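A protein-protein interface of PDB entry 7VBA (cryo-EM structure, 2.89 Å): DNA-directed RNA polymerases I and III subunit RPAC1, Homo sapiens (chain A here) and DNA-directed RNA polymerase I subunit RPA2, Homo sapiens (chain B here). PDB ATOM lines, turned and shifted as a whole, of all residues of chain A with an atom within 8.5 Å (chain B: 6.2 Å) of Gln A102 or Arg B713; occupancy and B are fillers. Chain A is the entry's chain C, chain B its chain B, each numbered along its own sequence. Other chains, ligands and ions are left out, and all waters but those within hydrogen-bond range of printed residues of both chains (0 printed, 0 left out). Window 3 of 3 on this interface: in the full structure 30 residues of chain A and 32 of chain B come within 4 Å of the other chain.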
ATOM      1  N   VAL A  94      17.113 -30.792  10.675  1.00  0.00           N
ATOM      2  CA  VAL A  94      17.029 -29.339  10.989  1.00  0.00           C
ATOM      3  C   VAL A  94      18.429 -28.766  11.163  1.00  0.00           C
ATOM      4  O   VAL A  94      19.052 -29.075  12.161  1.00  0.00           O
ATOM      5  CB  VAL A  94      16.174 -29.101  12.243  1.00  0.00           C
ATOM      6  CG1 VAL A  94      15.555 -27.718  12.239  1.00  0.00           C
ATOM      7  CG2 VAL A  94      15.086 -30.147  12.372  1.00  0.00           C
ATOM      8  N   ASN A  97      17.268 -23.637  13.650  1.00  0.00           N
ATOM      9  CA  ASN A  97      15.849 -23.316  13.786  1.00  0.00           C
ATOM     10  C   ASN A  97      15.716 -22.326  14.935  1.00  0.00           C
ATOM     11  O   ASN A  97      15.679 -22.726  16.102  1.00  0.00           O
ATOM     12  CB  ASN A  97      15.019 -24.568  14.043  1.00  0.00           C
ATOM     13  CG  ASN A  97      13.545 -24.267  14.220  1.00  0.00           C
ATOM     14  OD1 ASN A  97      13.128 -23.113  14.196  1.00  0.00           O
ATOM     15  ND2 ASN A  97      12.750 -25.309  14.412  1.00  0.00           N
ATOM     16  N   THR A  98      15.644 -21.036  14.611  1.00  0.00           N
ATOM     17  CA  THR A  98      15.476 -19.991  15.612  1.00  0.00           C
ATOM     18  C   THR A  98      14.032 -19.514  15.705  1.00  0.00           C
ATOM     19  O   THR A  98      13.782 -18.354  16.041  1.00  0.00           O
ATOM     20  CB  THR A  98      16.409 -18.818  15.322  1.00  0.00           C
ATOM     21  OG1 THR A  98      16.191 -18.349  13.987  1.00  0.00           O
ATOM     22  CG2 THR A  98      17.858 -19.243  15.469  1.00  0.00           C
ATOM     23  N   SER A  99      13.077 -20.391  15.417  1.00  0.00           N
ATOM     24  CA  SER A  99      11.671 -20.037  15.462  1.00  0.00           C
ATOM     25  C   SER A  99      11.104 -20.247  16.863  1.00  0.00           C
ATOM     26  O   SER A  99      11.737 -20.838  17.741  1.00  0.00           O
ATOM     27  CB  SER A  99      10.879 -20.863  14.452  1.00  0.00           C
ATOM     28  OG  SER A  99      11.055 -20.373  13.138  1.00  0.00           O
ATOM     29  N   ILE A 100       9.886 -19.743  17.066  1.00  0.00           N
ATOM     30  CA  ILE A 100       9.166 -20.025  18.303  1.00  0.00           C
ATOM     31  C   ILE A 100       8.657 -21.459  18.308  1.00  0.00           C
ATOM     32  O   ILE A 100       8.537 -22.079  19.371  1.00  0.00           O
ATOM     33  CB  ILE A 100       8.017 -19.018  18.496  1.00  0.00           C
ATOM     34  CG1 ILE A 100       8.574 -17.652  18.878  1.00  0.00           C
ATOM     35  CG2 ILE A 100       7.056 -19.502  19.559  1.00  0.00           C
ATOM     36  CD1 ILE A 100       9.452 -17.685  20.103  1.00  0.00           C
ATOM     37  N   VAL A 101       8.349 -22.007  17.133  1.00  0.00           N
ATOM     38  CA  VAL A 101       7.891 -23.388  17.040  1.00  0.00           C
ATOM     39  C   VAL A 101       9.066 -24.327  17.276  1.00  0.00           C
ATOM     40  O   VAL A 101      10.134 -24.176  16.673  1.00  0.00           O
ATOM     41  CB  VAL A 101       7.236 -23.644  15.676  1.00  0.00           C
ATOM     42  CG1 VAL A 101       6.474 -24.952  15.697  1.00  0.00           C
ATOM     43  CG2 VAL A 101       6.310 -22.496  15.313  1.00  0.00           C
ATOM     44  N   GLN A 102       8.868 -25.306  18.154  1.00  0.00           N
ATOM     45  CA  GLN A 102       9.937 -26.211  18.540  1.00  0.00           C
ATOM     46  C   GLN A 102      10.371 -27.062  17.348  1.00  0.00           C
ATOM     47  O   GLN A 102       9.791 -27.011  16.262  1.00  0.00           O
ATOM     48  CB  GLN A 102       9.486 -27.095  19.697  1.00  0.00           C
ATOM     49  CG  GLN A 102       9.548 -26.419  21.049  1.00  0.00           C
ATOM     50  CD  GLN A 102       8.480 -25.367  21.221  1.00  0.00           C
ATOM     51  OE1 GLN A 102       8.775 -24.177  21.312  1.00  0.00           O
ATOM     52  NE2 GLN A 102       7.226 -25.799  21.276  1.00  0.00           N
ATOM     53  N   ASP A 103      11.416 -27.863  17.562  1.00  0.00           N
ATOM     54  CA  ASP A 103      11.917 -28.737  16.508  1.00  0.00           C
ATOM     55  C   ASP A 103      11.053 -29.983  16.366  1.00  0.00           C
ATOM     56  O   ASP A 103      10.693 -30.375  15.251  1.00  0.00           O
ATOM     57  CB  ASP A 103      13.366 -29.126  16.794  1.00  0.00           C
ATOM     58  CG  ASP A 103      14.338 -28.007  16.496  1.00  0.00           C
ATOM     59  OD1 ASP A 103      14.074 -27.228  15.559  1.00  0.00           O
ATOM     60  OD2 ASP A 103      15.368 -27.907  17.196  1.00  0.00           O
ATOM     61  N   GLU A 104      10.706 -30.615  17.488  1.00  0.00           N
ATOM     62  CA  GLU A 104       9.842 -31.787  17.435  1.00  0.00           C
ATOM     63  C   GLU A 104       8.432 -31.425  16.993  1.00  0.00           C
ATOM     64  O   GLU A 104       7.805 -32.179  16.241  1.00  0.00           O
ATOM     65  CB  GLU A 104       9.817 -32.470  18.800  1.00  0.00           C
ATOM     66  CG  GLU A 104       9.505 -31.528  19.950  1.00  0.00           C
ATOM     67  CD  GLU A 104      10.753 -31.002  20.632  1.00  0.00           C
ATOM     68  OE1 GLU A 104      10.854 -31.128  21.870  1.00  0.00           O
ATOM     69  OE2 GLU A 104      11.632 -30.460  19.931  1.00  0.00           O
ATOM     70  N   ILE A 105       7.926 -30.270  17.428  1.00  0.00           N
ATOM     71  CA  ILE A 105       6.600 -29.832  17.007  1.00  0.00           C
ATOM     72  C   ILE A 105       6.606 -29.442  15.536  1.00  0.00           C
ATOM     73  O   ILE A 105       5.627 -29.667  14.818  1.00  0.00           O
ATOM     74  CB  ILE A 105       6.117 -28.677  17.899  1.00  0.00           C
ATOM     75  CG1 ILE A 105       5.849 -29.187  19.314  1.00  0.00           C
ATOM     76  CG2 ILE A 105       4.886 -28.023  17.302  1.00  0.00           C
ATOM     77  CD1 ILE A 105       7.065 -29.191  20.198  1.00  0.00           C
ATOM     78  N   LEU A 106       7.707 -28.864  15.061  1.00  0.00           N
ATOM     79  CA  LEU A 106       7.825 -28.578  13.636  1.00  0.00           C
ATOM     80  C   LEU A 106       7.859 -29.862  12.821  1.00  0.00           C
ATOM     81  O   LEU A 106       7.218 -29.952  11.770  1.00  0.00           O
ATOM     82  CB  LEU A 106       9.074 -27.742  13.371  1.00  0.00           C
ATOM     83  CG  LEU A 106       9.034 -26.849  12.135  1.00  0.00           C
ATOM     84  CD1 LEU A 106       7.795 -25.975  12.158  1.00  0.00           C
ATOM     85  CD2 LEU A 106      10.284 -26.003  12.070  1.00  0.00           C
ATOM     86  N   ALA A 107       8.599 -30.869  13.289  1.00  0.00           N
ATOM     87  CA  ALA A 107       8.620 -32.150  12.593  1.00  0.00           C
ATOM     88  C   ALA A 107       7.232 -32.773  12.547  1.00  0.00           C
ATOM     89  O   ALA A 107       6.796 -33.266  11.498  1.00  0.00           O
ATOM     90  CB  ALA A 107       9.613 -33.093  13.266  1.00  0.00           C
ATOM     91  N   HIS A 108       6.521 -32.761  13.674  1.00  0.00           N
ATOM     92  CA  HIS A 108       5.145 -33.244  13.678  1.00  0.00           C
ATOM     93  C   HIS A 108       4.303 -32.500  12.651  1.00  0.00           C
ATOM     94  O   HIS A 108       3.695 -33.114  11.768  1.00  0.00           O
ATOM     95  CB  HIS A 108       4.540 -33.106  15.073  1.00  0.00           C
ATOM     96  CG  HIS A 108       3.174 -33.700  15.197  1.00  0.00           C
ATOM     97  ND1 HIS A 108       2.951 -35.060  15.189  1.00  0.00           N
ATOM     98  CD2 HIS A 108       1.957 -33.122  15.326  1.00  0.00           C
ATOM     99  CE1 HIS A 108       1.657 -35.293  15.308  1.00  0.00           C
ATOM    100  NE2 HIS A 108       1.032 -34.133  15.392  1.00  0.00           N
ATOM    101  N   ARG A 109       4.257 -31.168  12.747  1.00  0.00           N
ATOM    102  CA  ARG A 109       3.459 -30.384  11.811  1.00  0.00           C
ATOM    103  C   ARG A 109       3.824 -30.680  10.364  1.00  0.00           C
ATOM    104  O   ARG A 109       2.961 -30.620   9.485  1.00  0.00           O
ATOM    105  CB  ARG A 109       3.629 -28.893  12.092  1.00  0.00           C
ATOM    106  CG  ARG A 109       2.568 -28.309  12.997  1.00  0.00           C
ATOM    107  CD  ARG A 109       2.753 -26.822  13.163  1.00  0.00           C
ATOM    108  NE  ARG A 109       1.987 -26.066  12.183  1.00  0.00           N
ATOM    109  CZ  ARG A 109       0.688 -25.815  12.283  1.00  0.00           C
ATOM    110  NH1 ARG A 109       0.004 -26.271  13.320  1.00  0.00           N
ATOM    111  NH2 ARG A 109       0.071 -25.116  11.343  1.00  0.00           N
ATOM    112  N   LEU A 110       5.092 -30.991  10.094  1.00  0.00           N
ATOM    113  CA  LEU A 110       5.505 -31.283   8.727  1.00  0.00           C
ATOM    114  C   LEU A 110       5.077 -32.672   8.285  1.00  0.00           C
ATOM    115  O   LEU A 110       4.857 -32.895   7.091  1.00  0.00           O
ATOM    116  CB  LEU A 110       7.019 -31.141   8.591  1.00  0.00           C
ATOM    117  CG  LEU A 110       7.570 -29.719   8.628  1.00  0.00           C
ATOM    118  CD1 LEU A 110       9.079 -29.753   8.576  1.00  0.00           C
ATOM    119  CD2 LEU A 110       7.011 -28.901   7.485  1.00  0.00           C
ATOM    120  N   ILE A 199       2.742 -23.077   8.315  1.00  0.00           N
ATOM    121  CA  ILE A 199       3.678 -23.955   9.006  1.00  0.00           C
ATOM    122  C   ILE A 199       4.206 -23.310  10.279  1.00  0.00           C
ATOM    123  O   ILE A 199       4.338 -23.969  11.313  1.00  0.00           O
ATOM    124  CB  ILE A 199       4.830 -24.347   8.059  1.00  0.00           C
ATOM    125  CG1 ILE A 199       4.307 -25.186   6.897  1.00  0.00           C
ATOM    126  CG2 ILE A 199       5.904 -25.104   8.814  1.00  0.00           C
ATOM    127  CD1 ILE A 199       5.362 -25.513   5.874  1.00  0.00           C
ATOM    128  N   ALA A 200       4.524 -22.022  10.232  1.00  0.00           N
ATOM    129  CA  ALA A 200       5.086 -21.331  11.384  1.00  0.00           C
ATOM    130  C   ALA A 200       4.895 -19.834  11.194  1.00  0.00           C
ATOM    131  O   ALA A 200       4.337 -19.378  10.193  1.00  0.00           O
ATOM    132  CB  ALA A 200       6.562 -21.686  11.571  1.00  0.00           C
ATOM    133  N   ILE A 208      14.276 -20.500   9.566  1.00  0.00           N
ATOM    134  CA  ILE A 208      14.023 -21.934   9.503  1.00  0.00           C
ATOM    135  C   ILE A 208      14.806 -22.511   8.333  1.00  0.00           C
ATOM    136  O   ILE A 208      14.886 -21.895   7.265  1.00  0.00           O
ATOM    137  CB  ILE A 208      12.522 -22.248   9.360  1.00  0.00           C
ATOM    138  CG1 ILE A 208      11.761 -21.785  10.599  1.00  0.00           C
ATOM    139  CG2 ILE A 208      12.315 -23.729   9.150  1.00  0.00           C
ATOM    140  CD1 ILE A 208      10.277 -22.025  10.519  1.00  0.00           C
ATOM    141  N   LEU A 210      15.617 -26.618   6.892  1.00  0.00           N
ATOM    142  CA  LEU A 210      15.457 -28.045   7.130  1.00  0.00           C
ATOM    143  C   LEU A 210      15.257 -28.796   5.818  1.00  0.00           C
ATOM    144  O   LEU A 210      14.895 -28.221   4.789  1.00  0.00           O
ATOM    145  CB  LEU A 210      14.289 -28.310   8.087  1.00  0.00           C
ATOM    146  CG  LEU A 210      12.923 -27.763   7.680  1.00  0.00           C
ATOM    147  CD1 LEU A 210      12.185 -28.767   6.825  1.00  0.00           C
ATOM    148  CD2 LEU A 210      12.112 -27.408   8.906  1.00  0.00           C
ATOM    149  N   MET B 696      -2.089 -30.075  32.909  1.00  0.00           N
ATOM    150  CA  MET B 696      -1.104 -29.635  31.933  1.00  0.00           C
ATOM    151  C   MET B 696      -1.769 -28.629  31.005  1.00  0.00           C
ATOM    152  O   MET B 696      -2.709 -28.972  30.283  1.00  0.00           O
ATOM    153  CB  MET B 696      -0.578 -30.833  31.150  1.00  0.00           C
ATOM    154  CG  MET B 696       0.746 -30.617  30.460  1.00  0.00           C
ATOM    155  SD  MET B 696       1.335 -32.155  29.739  1.00  0.00           S
ATOM    156  CE  MET B 696       2.998 -31.713  29.268  1.00  0.00           C
ATOM    157  N   GLY B 697      -1.303 -27.386  31.037  1.00  0.00           N
ATOM    158  CA  GLY B 697      -1.911 -26.353  30.227  1.00  0.00           C
ATOM    159  C   GLY B 697      -0.900 -25.406  29.625  1.00  0.00           C
ATOM    160  O   GLY B 697       0.211 -25.811  29.278  1.00  0.00           O
ATOM    161  N   PHE B 698      -1.278 -24.138  29.486  1.00  0.00           N
ATOM    162  CA  PHE B 698      -0.359 -23.102  29.044  1.00  0.00           C
ATOM    163  C   PHE B 698      -0.010 -22.251  30.256  1.00  0.00           C
ATOM    164  O   PHE B 698      -0.817 -21.407  30.667  1.00  0.00           O
ATOM    165  CB  PHE B 698      -0.992 -22.250  27.943  1.00  0.00           C
ATOM    166  CG  PHE B 698       0.006 -21.569  27.059  1.00  0.00           C
ATOM    167  CD1 PHE B 698       0.779 -22.302  26.180  1.00  0.00           C
ATOM    168  CD2 PHE B 698       0.171 -20.199  27.103  1.00  0.00           C
ATOM    169  CE1 PHE B 698       1.699 -21.684  25.367  1.00  0.00           C
ATOM    170  CE2 PHE B 698       1.092 -19.576  26.289  1.00  0.00           C
ATOM    171  CZ  PHE B 698       1.857 -20.321  25.421  1.00  0.00           C
ATOM    172  N   PRO B 699       1.158 -22.432  30.867  1.00  0.00           N
ATOM    173  CA  PRO B 699       1.396 -21.840  32.188  1.00  0.00           C
ATOM    174  C   PRO B 699       1.802 -20.378  32.141  1.00  0.00           C
ATOM    175  O   PRO B 699       1.536 -19.633  33.087  1.00  0.00           O
ATOM    176  CB  PRO B 699       2.519 -22.713  32.758  1.00  0.00           C
ATOM    177  CG  PRO B 699       3.212 -23.295  31.569  1.00  0.00           C
ATOM    178  CD  PRO B 699       2.344 -23.133  30.354  1.00  0.00           C
ATOM    179  N   TYR B 703       8.926 -17.984  28.157  1.00  0.00           N
ATOM    180  CA  TYR B 703       9.983 -18.975  28.213  1.00  0.00           C
ATOM    181  C   TYR B 703      11.286 -18.299  27.822  1.00  0.00           C
ATOM    182  O   TYR B 703      11.299 -17.151  27.369  1.00  0.00           O
ATOM    183  CB  TYR B 703       9.674 -20.144  27.281  1.00  0.00           C
ATOM    184  CG  TYR B 703       8.386 -20.839  27.635  1.00  0.00           C
ATOM    185  CD1 TYR B 703       8.342 -21.784  28.646  1.00  0.00           C
ATOM    186  CD2 TYR B 703       7.203 -20.521  26.986  1.00  0.00           C
ATOM    187  CE1 TYR B 703       7.161 -22.409  28.984  1.00  0.00           C
ATOM    188  CE2 TYR B 703       6.016 -21.137  27.322  1.00  0.00           C
ATOM    189  CZ  TYR B 703       6.000 -22.080  28.321  1.00  0.00           C
ATOM    190  OH  TYR B 703       4.819 -22.696  28.653  1.00  0.00           O
ATOM    191  N   LEU B 711       8.192 -27.450  34.241  1.00  0.00           N
ATOM    192  CA  LEU B 711       7.216 -26.532  33.664  1.00  0.00           C
ATOM    193  C   LEU B 711       6.480 -27.259  32.549  1.00  0.00           C
ATOM    194  O   LEU B 711       7.012 -27.400  31.447  1.00  0.00           O
ATOM    195  CB  LEU B 711       7.902 -25.270  33.159  1.00  0.00           C
ATOM    196  CG  LEU B 711       6.996 -24.109  32.775  1.00  0.00           C
ATOM    197  CD1 LEU B 711       7.725 -22.796  32.953  1.00  0.00           C
ATOM    198  CD2 LEU B 711       6.547 -24.275  31.346  1.00  0.00           C
ATOM    199  N   TYR B 712       5.258 -27.707  32.832  1.00  0.00           N
ATOM    200  CA  TYR B 712       4.472 -28.501  31.896  1.00  0.00           C
ATOM    201  C   TYR B 712       3.727 -27.590  30.932  1.00  0.00           C
ATOM    202  O   TYR B 712       3.047 -26.654  31.357  1.00  0.00           O
ATOM    203  CB  TYR B 712       3.477 -29.384  32.648  1.00  0.00           C
ATOM    204  CG  TYR B 712       4.118 -30.286  33.668  1.00  0.00           C
ATOM    205  CD1 TYR B 712       4.396 -29.832  34.948  1.00  0.00           C
ATOM    206  CD2 TYR B 712       4.449 -31.591  33.351  1.00  0.00           C
ATOM    207  CE1 TYR B 712       4.987 -30.653  35.879  1.00  0.00           C
ATOM    208  CE2 TYR B 712       5.036 -32.418  34.274  1.00  0.00           C
ATOM    209  CZ  TYR B 712       5.305 -31.948  35.535  1.00  0.00           C
ATOM    210  OH  TYR B 712       5.895 -32.789  36.452  1.00  0.00           O
ATOM    211  N   ARG B 713       3.837 -27.881  29.638  1.00  0.00           N
ATOM    212  CA  ARG B 713       3.214 -27.064  28.607  1.00  0.00           C
ATOM    213  C   ARG B 713       2.404 -27.940  27.666  1.00  0.00           C
ATOM    214  O   ARG B 713       2.891 -28.976  27.202  1.00  0.00           O
ATOM    215  CB  ARG B 713       4.266 -26.286  27.817  1.00  0.00           C
ATOM    216  CG  ARG B 713       3.697 -25.471  26.680  1.00  0.00           C
ATOM    217  CD  ARG B 713       4.805 -24.897  25.835  1.00  0.00           C
ATOM    218  NE  ARG B 713       4.292 -24.112  24.722  1.00  0.00           N
ATOM    219  CZ  ARG B 713       5.035 -23.292  23.989  1.00  0.00           C
ATOM    220  NH1 ARG B 713       6.324 -23.151  24.255  1.00  0.00           N
ATOM    221  NH2 ARG B 713       4.488 -22.611  22.994  1.00  0.00           N
ATOM    222  N   LEU B 714       1.176 -27.524  27.385  1.00  0.00           N
ATOM    223  CA  LEU B 714       0.339 -28.171  26.387  1.00  0.00           C
ATOM    224  C   LEU B 714       0.450 -27.421  25.067  1.00  0.00           C
ATOM    225  O   LEU B 714       0.374 -26.190  25.034  1.00  0.00           O
ATOM    226  CB  LEU B 714      -1.113 -28.207  26.859  1.00  0.00           C
ATOM    227  CG  LEU B 714      -2.134 -28.982  26.036  1.00  0.00           C
ATOM    228  CD1 LEU B 714      -2.134 -30.441  26.433  1.00  0.00           C
ATOM    229  CD2 LEU B 714      -3.499 -28.370  26.246  1.00  0.00           C
ATOM    230  N   GLN B 715       0.620 -28.167  23.975  1.00  0.00           N
ATOM    231  CA  GLN B 715       0.966 -27.533  22.706  1.00  0.00           C
ATOM    232  C   GLN B 715      -0.169 -26.661  22.181  1.00  0.00           C
ATOM    233  O   GLN B 715      -0.022 -25.441  22.060  1.00  0.00           O
ATOM    234  CB  GLN B 715       1.355 -28.591  21.674  1.00  0.00           C
ATOM    235  CG  GLN B 715       2.741 -29.151  21.895  1.00  0.00           C
ATOM    236  CD  GLN B 715       3.756 -28.061  22.161  1.00  0.00           C
ATOM    237  OE1 GLN B 715       3.844 -27.083  21.417  1.00  0.00           O
ATOM    238  NE2 GLN B 715       4.520 -28.213  23.237  1.00  0.00           N
ATOM    239  N   HIS B 770      -0.971 -33.265  22.777  1.00  0.00           N
ATOM    240  CA  HIS B 770       0.476 -33.369  22.869  1.00  0.00           C
ATOM    241  C   HIS B 770       1.010 -32.327  23.844  1.00  0.00           C
ATOM    242  O   HIS B 770       0.398 -31.282  24.064  1.00  0.00           O
ATOM    243  CB  HIS B 770       1.108 -33.188  21.493  1.00  0.00           C
ATOM    244  CG  HIS B 770       0.948 -34.375  20.594  1.00  0.00           C
ATOM    245  ND1 HIS B 770       1.371 -34.376  19.284  1.00  0.00           N
ATOM    246  CD2 HIS B 770       0.416 -35.598  20.819  1.00  0.00           C
ATOM    247  CE1 HIS B 770       1.105 -35.550  18.739  1.00  0.00           C
ATOM    248  NE2 HIS B 770       0.525 -36.309  19.649  1.00  0.00           N
ATOM    249  N   GLY B 771       2.164 -32.617  24.435  1.00  0.00           N
ATOM    250  CA  GLY B 771       2.679 -31.744  25.469  1.00  0.00           C
ATOM    251  C   GLY B 771       4.181 -31.852  25.600  1.00  0.00           C
ATOM    252  O   GLY B 771       4.850 -32.536  24.823  1.00  0.00           O
ATOM    253  N   SER B 772       4.707 -31.153  26.602  1.00  0.00           N
ATOM    254  CA  SER B 772       6.141 -31.119  26.845  1.00  0.00           C
ATOM    255  C   SER B 772       6.400 -30.696  28.282  1.00  0.00           C
ATOM    256  O   SER B 772       5.528 -30.155  28.963  1.00  0.00           O
ATOM    257  CB  SER B 772       6.852 -30.167  25.879  1.00  0.00           C
ATOM    258  OG  SER B 772       6.730 -30.603  24.539  1.00  0.00           O
ATOM    259  N   VAL B 773       7.624 -30.946  28.732  1.00  0.00           N
ATOM    260  CA  VAL B 773       8.094 -30.510  30.040  1.00  0.00           C
ATOM    261  C   VAL B 773       9.428 -29.806  29.852  1.00  0.00           C
ATOM    262  O   VAL B 773      10.244 -30.213  29.021  1.00  0.00           O
ATOM    263  CB  VAL B 773       8.233 -31.689  31.022  1.00  0.00           C
ATOM    264  CG1 VAL B 773       8.526 -31.184  32.415  1.00  0.00           C
ATOM    265  CG2 VAL B 773       6.973 -32.523  31.019  1.00  0.00           C
ATOM    266  N   TYR B 774       9.648 -28.746  30.617  1.00  0.00           N
ATOM    267  CA  TYR B 774      10.897 -27.995  30.583  1.00  0.00           C
ATOM    268  C   TYR B 774      11.612 -28.206  31.908  1.00  0.00           C
ATOM    269  O   TYR B 774      11.162 -27.715  32.946  1.00  0.00           O
ATOM    270  CB  TYR B 774      10.642 -26.511  30.333  1.00  0.00           C
ATOM    271  CG  TYR B 774      10.052 -26.205  28.981  1.00  0.00           C
ATOM    272  CD1 TYR B 774       8.715 -26.444  28.717  1.00  0.00           C
ATOM    273  CD2 TYR B 774      10.833 -25.668  27.971  1.00  0.00           C
ATOM    274  CE1 TYR B 774       8.171 -26.164  27.486  1.00  0.00           C
ATOM    275  CE2 TYR B 774      10.298 -25.384  26.735  1.00  0.00           C
ATOM    276  CZ  TYR B 774       8.967 -25.634  26.498  1.00  0.00           C
ATOM    277  OH  TYR B 774       8.426 -25.352  25.267  1.00  0.00           O
ATOM    278  N   ARG B 872      14.235 -29.922  27.122  1.00  0.00           N
ATOM    279  CA  ARG B 872      12.848 -30.089  26.713  1.00  0.00           C
ATOM    280  C   ARG B 872      12.578 -31.576  26.549  1.00  0.00           C
ATOM    281  O   ARG B 872      13.297 -32.262  25.816  1.00  0.00           O
ATOM    282  CB  ARG B 872      12.573 -29.336  25.413  1.00  0.00           C
ATOM    283  CG  ARG B 872      11.139 -28.903  25.223  1.00  0.00           C
ATOM    284  CD  ARG B 872      11.064 -27.780  24.210  1.00  0.00           C
ATOM    285  NE  ARG B 872      11.780 -28.119  22.985  1.00  0.00           N
ATOM    286  CZ  ARG B 872      12.493 -27.255  22.273  1.00  0.00           C
ATOM    287  NH1 ARG B 872      12.589 -25.993  22.664  1.00  0.00           N
ATOM    288  NH2 ARG B 872      13.113 -27.653  21.173  1.00  0.00           N
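NE of Arg B872 lies within salt-bridge range of OE1 of Glu A104.
Hydrophobic or aromatic side chains of chain B within 4 Å of the printed part of chain A: His B770. Printed residues of chain A that touch a printed residue of chain B: Gln A102, Asp A103, Glu A104, Ile A105 and His A108. Hydrophobic or aromatic side chains of chain A within 4 Å of the printed part of chain B: Ile A105 and His A108. Among the printed residues, 7 pairs touch across the chains. Among the printed residues, Asp or Glu carboxylates within 4 Å of a Lys or Arg side-chain nitrogen of the other chain: Glu A104 with Arg B872 (3.3 Å).
Gln A102 touches just these residues of chain B: Arg B713, Gln B715 and Arg B872. Arg B713 touches one residue of chain A. Of the printed residues of chain A, Gln B715 touches Gln A102 and Ile A105. Printed residues of chain B within 4 Å of His A108: His B770. Printed residues of chain B within 4 Å of Glu A104: Arg B872. Printed residues of chain B within 4 Å of Ile A105: Gln B715 (3.6 Å). Gly B771 touches none of the printed residues of chain A. Ile A100 touches none of the printed residues of chain B. The nearest residue of chain A that does not touch Arg B713 is Ile A100 (5.3 Å). The nearest printed residue of chain B that does not touch His A108 is Gln B715 (7.7 Å).
The backbone carbonyl oxygen of Ile A100 sits close to the side-chain amide oxygen of Gln A102 (2.9 Å). ND2 of Asn A97 lies within hydrogen-bond range of OD1 of Asp A103 (2.6 Å). The guanidinium group of Arg B713 is in hydrogen-bond range of the side-chain hydroxyl of Tyr B774 (3.2 Å). The backbone NH (N) of Ser B772 is in hydrogen-bond range of the backbone carbonyl oxygen (O) of Arg B713, at 2.9 Å. O of His B770 sits at hydrogen-bond distance from N of Gln B715 (3.1 Å).
Among the printed residues, merely in contact across the chains: Gln A102 with Arg B713, Gln A102 with Gln B715, Gln A102 with Arg B872, Asp A103 with Arg B872, Ile A105 with Gln B715 and His A108 with His B770.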
